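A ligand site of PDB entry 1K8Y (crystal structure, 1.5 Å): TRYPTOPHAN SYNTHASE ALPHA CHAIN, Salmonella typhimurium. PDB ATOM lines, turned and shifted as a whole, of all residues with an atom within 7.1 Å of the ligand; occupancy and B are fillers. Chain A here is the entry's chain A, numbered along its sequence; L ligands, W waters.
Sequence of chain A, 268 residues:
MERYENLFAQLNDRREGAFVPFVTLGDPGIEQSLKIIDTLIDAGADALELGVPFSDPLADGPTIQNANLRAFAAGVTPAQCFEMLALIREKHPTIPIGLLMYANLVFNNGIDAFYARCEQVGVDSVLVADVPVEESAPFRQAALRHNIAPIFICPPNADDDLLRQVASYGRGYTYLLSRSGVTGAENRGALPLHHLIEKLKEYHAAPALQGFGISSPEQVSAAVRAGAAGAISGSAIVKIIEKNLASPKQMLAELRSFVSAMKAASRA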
ATOM      1  N   PHE A  22      20.977 -11.889   8.592  1.00  0.00           N
ATOM      2  CA  PHE A  22      20.796 -12.527   9.837  1.00  0.00           C
ATOM      3  C   PHE A  22      21.661 -11.970  10.912  1.00  0.00           C
ATOM      4  O   PHE A  22      22.880 -11.783  10.648  1.00  0.00           O
ATOM      5  CB  PHE A  22      21.045 -14.107   9.749  1.00  0.00           C
ATOM      6  CG  PHE A  22      21.157 -14.734  11.149  1.00  0.00           C
ATOM      7  CD1 PHE A  22      22.375 -14.744  11.855  1.00  0.00           C
ATOM      8  CD2 PHE A  22      20.049 -15.305  11.810  1.00  0.00           C
ATOM      9  CE1 PHE A  22      22.441 -15.338  13.159  1.00  0.00           C
ATOM     10  CE2 PHE A  22      20.126 -15.815  13.060  1.00  0.00           C
ATOM     11  CZ  PHE A  22      21.328 -15.869  13.747  1.00  0.00           C
ATOM     12  N   VAL A  23      21.146 -11.759  12.143  1.00  0.00           N
ATOM     13  CA  VAL A  23      22.012 -11.484  13.351  1.00  0.00           C
ATOM     14  C   VAL A  23      21.434 -12.243  14.519  1.00  0.00           C
ATOM     15  O   VAL A  23      20.240 -12.612  14.528  1.00  0.00           O
ATOM     16  CB  VAL A  23      22.292  -9.996  13.722  1.00  0.00           C
ATOM     17  CG1 VAL A  23      22.995  -9.276  12.603  1.00  0.00           C
ATOM     18  CG2 VAL A  23      20.877  -9.367  14.018  1.00  0.00           C
ATOM     19  N   GLU A  49      16.351 -11.825   9.547  1.00  0.00           N
ATOM     20  CA  GLU A  49      16.209 -13.133  10.250  1.00  0.00           C
ATOM     21  C   GLU A  49      16.969 -12.923  11.586  1.00  0.00           C
ATOM     22  O   GLU A  49      18.104 -12.375  11.532  1.00  0.00           O
ATOM     23  CB  GLU A  49      16.854 -14.273   9.375  1.00  0.00           C
ATOM     24  CG  GLU A  49      16.038 -14.690   8.152  1.00  0.00           C
ATOM     25  CD  GLU A  49      14.636 -15.248   8.623  1.00  0.00           C
ATOM     26  OE1 GLU A  49      14.705 -15.951   9.672  1.00  0.00           O
ATOM     27  OE2 GLU A  49      13.613 -14.946   8.001  1.00  0.00           O
ATOM     28  N   ASP A  60      24.619 -24.705  13.821  1.00  0.00           N
ATOM     29  CA  ASP A  60      25.287 -23.513  13.474  1.00  0.00           C
ATOM     30  C   ASP A  60      26.841 -23.677  13.451  1.00  0.00           C
ATOM     31  O   ASP A  60      27.345 -24.465  14.339  1.00  0.00           O
ATOM     32  CB  ASP A  60      24.982 -22.453  14.556  1.00  0.00           C
ATOM     33  CG  ASP A  60      23.709 -21.675  14.224  1.00  0.00           C
ATOM     34  OD1 ASP A  60      23.678 -20.895  13.130  1.00  0.00           O
ATOM     35  OD2 ASP A  60      22.789 -21.859  15.023  1.00  0.00           O
ATOM     36  N   GLY A  61      27.578 -23.035  12.517  1.00  0.00           N
ATOM     37  CA  GLY A  61      29.023 -23.072  12.621  1.00  0.00           C
ATOM     38  C   GLY A  61      29.593 -22.066  13.565  1.00  0.00           C
ATOM     39  O   GLY A  61      28.943 -21.420  14.388  1.00  0.00           O
ATOM     40  N   THR A  63      31.012 -19.147  13.615  1.00  0.00           N
ATOM     41  CA  THR A  63      30.768 -17.677  13.738  1.00  0.00           C
ATOM     42  C   THR A  63      29.500 -17.424  14.567  1.00  0.00           C
ATOM     43  O   THR A  63      29.516 -16.600  15.451  1.00  0.00           O
ATOM     44  CB  THR A  63      30.538 -17.151  12.305  1.00  0.00           C
ATOM     45  OG1 THR A  63      31.782 -17.335  11.597  1.00  0.00           O
ATOM     46  CG2 THR A  63      30.359 -15.567  12.404  1.00  0.00           C
ATOM     47  N   ILE A  64      28.398 -18.194  14.220  1.00  0.00           N
ATOM     48  CA  ILE A  64      27.210 -18.007  15.041  1.00  0.00           C
ATOM     49  C   ILE A  64      27.317 -18.613  16.419  1.00  0.00           C
ATOM     50  O   ILE A  64      26.814 -18.131  17.382  1.00  0.00           O
ATOM     51  CB  ILE A  64      25.988 -18.458  14.180  1.00  0.00           C
ATOM     52  CG1 ILE A  64      25.904 -17.234  13.134  1.00  0.00           C
ATOM     53  CG2 ILE A  64      24.725 -18.375  14.937  1.00  0.00           C
ATOM     54  CD1 ILE A  64      25.155 -17.605  11.873  1.00  0.00           C
ATOM     55  N   LEU A 100      14.891 -17.411  13.935  1.00  0.00           N
ATOM     56  CA  LEU A 100      15.584 -18.749  13.767  1.00  0.00           C
ATOM     57  C   LEU A 100      15.724 -19.215  15.136  1.00  0.00           C
ATOM     58  O   LEU A 100      16.418 -18.676  15.979  1.00  0.00           O
ATOM     59  CB  LEU A 100      16.910 -18.525  13.130  1.00  0.00           C
ATOM     60  CG  LEU A 100      17.894 -19.707  12.821  1.00  0.00           C
ATOM     61  CD1 LEU A 100      17.215 -20.652  12.027  1.00  0.00           C
ATOM     62  CD2 LEU A 100      18.978 -19.125  11.910  1.00  0.00           C
ATOM     63  N   LEU A 127      11.622 -20.268  11.731  1.00  0.00           N
ATOM     64  CA  LEU A 127      12.309 -21.463  11.244  1.00  0.00           C
ATOM     65  C   LEU A 127      12.854 -22.151  12.485  1.00  0.00           C
ATOM     66  O   LEU A 127      13.658 -21.558  13.193  1.00  0.00           O
ATOM     67  CB  LEU A 127      13.490 -20.960  10.298  1.00  0.00           C
ATOM     68  CG  LEU A 127      13.956 -22.236   9.492  1.00  0.00           C
ATOM     69  CD1 LEU A 127      15.250 -21.613   8.640  1.00  0.00           C
ATOM     70  CD2 LEU A 127      14.538 -23.269  10.153  1.00  0.00           C
ATOM     71  N   TYR A 173       8.501 -17.716   3.012  1.00  0.00           N
ATOM     72  CA  TYR A 173       9.504 -18.023   2.041  1.00  0.00           C
ATOM     73  C   TYR A 173       9.943 -19.466   2.267  1.00  0.00           C
ATOM     74  O   TYR A 173       9.687 -20.037   3.325  1.00  0.00           O
ATOM     75  CB  TYR A 173      10.666 -17.007   2.112  1.00  0.00           C
ATOM     76  CG  TYR A 173      11.505 -17.119   3.348  1.00  0.00           C
ATOM     77  CD1 TYR A 173      11.109 -16.471   4.531  1.00  0.00           C
ATOM     78  CD2 TYR A 173      12.572 -17.856   3.434  1.00  0.00           C
ATOM     79  CE1 TYR A 173      11.939 -16.658   5.717  1.00  0.00           C
ATOM     80  CE2 TYR A 173      13.350 -17.957   4.483  1.00  0.00           C
ATOM     81  CZ  TYR A 173      13.067 -17.407   5.627  1.00  0.00           C
ATOM     82  OH  TYR A 173      13.904 -17.630   6.766  1.00  0.00           O
ATOM     83  N   TYR A 175      13.392 -21.686   2.638  1.00  0.00           N
ATOM     84  CA  TYR A 175      14.803 -21.481   2.864  1.00  0.00           C
ATOM     85  C   TYR A 175      15.523 -22.449   2.029  1.00  0.00           C
ATOM     86  O   TYR A 175      15.532 -23.671   2.320  1.00  0.00           O
ATOM     87  CB  TYR A 175      15.086 -21.669   4.342  1.00  0.00           C
ATOM     88  CG  TYR A 175      16.438 -21.078   4.804  1.00  0.00           C
ATOM     89  CD1 TYR A 175      17.581 -21.639   4.219  1.00  0.00           C
ATOM     90  CD2 TYR A 175      16.548 -20.096   5.810  1.00  0.00           C
ATOM     91  CE1 TYR A 175      18.836 -21.248   4.622  1.00  0.00           C
ATOM     92  CE2 TYR A 175      17.756 -19.709   6.158  1.00  0.00           C
ATOM     93  CZ  TYR A 175      18.879 -20.242   5.523  1.00  0.00           C
ATOM     94  OH  TYR A 175      20.164 -19.873   5.866  1.00  0.00           O
ATOM     95  N   LEU A 177      18.662 -24.172   0.935  1.00  0.00           N
ATOM     96  CA  LEU A 177      19.976 -24.213   1.536  1.00  0.00           C
ATOM     97  C   LEU A 177      20.947 -24.381   0.304  1.00  0.00           C
ATOM     98  O   LEU A 177      20.608 -24.990  -0.719  1.00  0.00           O
ATOM     99  CB  LEU A 177      20.089 -25.323   2.621  1.00  0.00           C
ATOM    100  CG  LEU A 177      21.375 -25.360   3.478  1.00  0.00           C
ATOM    101  CD1 LEU A 177      21.239 -24.376   4.644  1.00  0.00           C
ATOM    102  CD2 LEU A 177      21.846 -26.808   4.064  1.00  0.00           C
ATOM    103  N   GLY A 211      20.182 -19.494   1.057  1.00  0.00           N
ATOM    104  CA  GLY A 211      20.980 -19.212   2.249  1.00  0.00           C
ATOM    105  C   GLY A 211      22.083 -20.183   2.518  1.00  0.00           C
ATOM    106  O   GLY A 211      21.954 -21.349   1.998  1.00  0.00           O
ATOM    107  N   PHE A 212      23.081 -19.792   3.327  1.00  0.00           N
ATOM    108  CA  PHE A 212      24.392 -20.510   3.664  1.00  0.00           C
ATOM    109  C   PHE A 212      25.533 -20.097   2.769  1.00  0.00           C
ATOM    110  O   PHE A 212      25.555 -20.307   1.471  1.00  0.00           O
ATOM    111  CB  PHE A 212      24.263 -22.126   3.683  1.00  0.00           C
ATOM    112  N   GLY A 213      26.515 -19.512   3.413  1.00  0.00           N
ATOM    113  CA  GLY A 213      27.626 -19.119   2.520  1.00  0.00           C
ATOM    114  C   GLY A 213      27.421 -17.729   1.760  1.00  0.00           C
ATOM    115  O   GLY A 213      28.462 -17.444   1.101  1.00  0.00           O
ATOM    116  N   ILE A 214      26.245 -17.046   1.809  1.00  0.00           N
ATOM    117  CA  ILE A 214      26.215 -15.946   0.866  1.00  0.00           C
ATOM    118  C   ILE A 214      27.022 -14.826   1.525  1.00  0.00           C
ATOM    119  O   ILE A 214      26.628 -14.350   2.611  1.00  0.00           O
ATOM    120  CB  ILE A 214      24.791 -15.507   0.735  1.00  0.00           C
ATOM    121  CG1 ILE A 214      23.790 -16.546   0.235  1.00  0.00           C
ATOM    122  CG2 ILE A 214      24.695 -14.241  -0.053  1.00  0.00           C
ATOM    123  CD1 ILE A 214      24.121 -16.939  -1.252  1.00  0.00           C
ATOM    124  N   SER A 215      28.179 -14.388   0.964  1.00  0.00           N
ATOM    125  CA  SER A 215      28.949 -13.342   1.585  1.00  0.00           C
ATOM    126  C   SER A 215      29.475 -12.212   0.654  1.00  0.00           C
ATOM    127  O   SER A 215      30.257 -11.407   1.076  1.00  0.00           O
ATOM    128  CB  SER A 215      30.216 -13.996   2.278  1.00  0.00           C
ATOM    129  OG  SER A 215      31.036 -14.610   1.210  1.00  0.00           O
ATOM    130  N   ILE A 232      19.745 -14.852   1.773  1.00  0.00           N
ATOM    131  CA  ILE A 232      20.053 -14.481   3.174  1.00  0.00           C
ATOM    132  C   ILE A 232      21.493 -14.572   3.527  1.00  0.00           C
ATOM    133  O   ILE A 232      22.241 -15.496   3.057  1.00  0.00           O
ATOM    134  CB  ILE A 232      19.240 -15.609   4.014  1.00  0.00           C
ATOM    135  CG1 ILE A 232      17.734 -15.362   3.882  1.00  0.00           C
ATOM    136  CG2 ILE A 232      19.813 -15.553   5.559  1.00  0.00           C
ATOM    137  CD1 ILE A 232      16.949 -16.781   4.357  1.00  0.00           C
ATOM    138  N   SER A 233      22.069 -13.670   4.339  1.00  0.00           N
ATOM    139  CA  SER A 233      23.471 -13.737   4.758  1.00  0.00           C
ATOM    140  C   SER A 233      23.507 -13.508   6.261  1.00  0.00           C
ATOM    141  O   SER A 233      23.002 -12.555   6.772  1.00  0.00           O
ATOM    142  CB  SER A 233      24.154 -12.493   4.118  1.00  0.00           C
ATOM    143  OG  SER A 233      25.542 -12.414   4.404  1.00  0.00           O
ATOM    144  N   GLY A 234      24.228 -14.370   6.926  1.00  0.00           N
ATOM    145  CA  GLY A 234      24.377 -14.213   8.417  1.00  0.00           C
ATOM    146  C   GLY A 234      25.773 -14.245   8.845  1.00  0.00           C
ATOM    147  O   GLY A 234      26.172 -13.177   9.384  1.00  0.00           O
ATOM    148  N   SER A 235      26.509 -15.346   8.645  1.00  0.00           N
ATOM    149  CA  SER A 235      27.872 -15.264   9.149  1.00  0.00           C
ATOM    150  C   SER A 235      28.604 -14.074   8.665  1.00  0.00           C
ATOM    151  O   SER A 235      29.399 -13.502   9.413  1.00  0.00           O
ATOM    152  CB  SER A 235      28.602 -16.565   8.695  1.00  0.00           C
ATOM    153  OG  SER A 235      28.116 -17.635   9.413  1.00  0.00           O
ATOM    154  N   ALA A 236      28.411 -13.690   7.381  1.00  0.00           N
ATOM    155  CA  ALA A 236      29.174 -12.528   6.966  1.00  0.00           C
ATOM    156  C   ALA A 236      28.812 -11.287   7.700  1.00  0.00           C
ATOM    157  O   ALA A 236      29.720 -10.460   7.913  1.00  0.00           O
ATOM    158  CB  ALA A 236      28.999 -12.292   5.557  1.00  0.00           C
ATOM    159  N   ILE A 237      27.520 -11.140   8.128  1.00  0.00           N
ATOM    160  CA  ILE A 237      27.191  -9.948   8.846  1.00  0.00           C
ATOM    161  C   ILE A 237      27.806 -10.123  10.258  1.00  0.00           C
ATOM    162  O   ILE A 237      28.310  -9.202  10.879  1.00  0.00           O
ATOM    163  CB  ILE A 237      25.638  -9.942   8.987  1.00  0.00           C
ATOM    164  CG1 ILE A 237      24.945 -10.011   7.616  1.00  0.00           C
ATOM    165  CG2 ILE A 237      25.189  -8.753   9.956  1.00  0.00           C
ATOM    166  CD1 ILE A 237      24.855  -8.734   6.893  1.00  0.00           C
ATOM    167  N   VAL A 238      27.666 -11.374  10.786  1.00  0.00           N
ATOM    168  CA  VAL A 238      28.091 -11.547  12.227  1.00  0.00           C
ATOM    169  C   VAL A 238      29.657 -11.368  12.340  1.00  0.00           C
ATOM    170  O   VAL A 238      30.163 -10.888  13.395  1.00  0.00           O
ATOM    171  CB  VAL A 238      27.637 -12.946  12.689  1.00  0.00           C
ATOM    172  CG1 VAL A 238      28.075 -13.173  14.204  1.00  0.00           C
ATOM    173  CG2 VAL A 238      26.039 -12.944  12.737  1.00  0.00           C
HETATM  174  P1  LIG L   1      25.478 -18.188   6.775  1.00  0.00           P
HETATM  175  O1  LIG L   1      26.439 -19.200   6.061  1.00  0.00           O
HETATM  176  O2  LIG L   1      25.819 -17.990   8.357  1.00  0.00           O
HETATM  177  O3  LIG L   1      25.297 -16.860   5.910  1.00  0.00           O
HETATM  178  O4  LIG L   1      24.062 -18.886   6.678  1.00  0.00           O
HETATM  179  C1  LIG L   1      22.964 -18.066   7.159  1.00  0.00           C
HETATM  180  C2  LIG L   1      22.630 -18.597   8.633  1.00  0.00           C
HETATM  181  O5  LIG L   1      23.463 -17.769   9.410  1.00  0.00           O
HETATM  182  C3  LIG L   1      21.280 -18.065   9.298  1.00  0.00           C
HETATM  183  O6  LIG L   1      20.240 -18.475   8.289  1.00  0.00           O
HETATM  184  O   HOH W   1      20.611 -20.830  10.073  1.00  0.00           O
HETATM  185  O   HOH W   2      24.222 -17.384   3.593  1.00  0.00           O
HETATM  186  O   HOH W   3      27.294 -15.366   5.269  1.00  0.00           O
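CG of Phe 22 touches C3 of the ligand, at 3.8 Å. CD1 of Ile 64 touches O5 of the ligand (3.0 Å). Leu 100 touches the ligand (CD2 to C3, 3.6 Å). Phe 212 touches the ligand (CA to O1, 3.4 Å). Ser 233 touches the ligand (CA to O3, 3.8 Å). Hydrophobic or aromatic side chains within 4 Å of the ligand: Phe 22, Ile 64, Leu 100 and Tyr 175.
Water W3 lies within hydrogen-bond range of an oxygen (O3) of the ligand, the backbone NH (N) of Ala 236, the backbone carbonyl oxygen (O) of Ile 214 and the backbone NH (N) of Ser 235.
O of Ser 233 lies within hydrogen-bond range of N of Phe 22. OG of Ser 233 lies within hydrogen-bond range of O of Ile 214, at 2.9 Å.
O2 of the ligand is in hydrogen-bond range of N of Ser 235 (2.7 Å). An oxygen (O6) of the ligand sits at hydrogen-bond distance from the side-chain hydroxyl of Tyr 175, at 2.8 Å. The side-chain hydroxyl (OG) of Ser 235 sits at hydrogen-bond distance from an oxygen (O2) of the ligand (2.6 Å). N of Gly 234 lies within hydrogen-bond range of O3 of the ligand (2.9 Å). The backbone NH (N) of Gly 213 is in hydrogen-bond range of an oxygen (O1) of the ligand.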
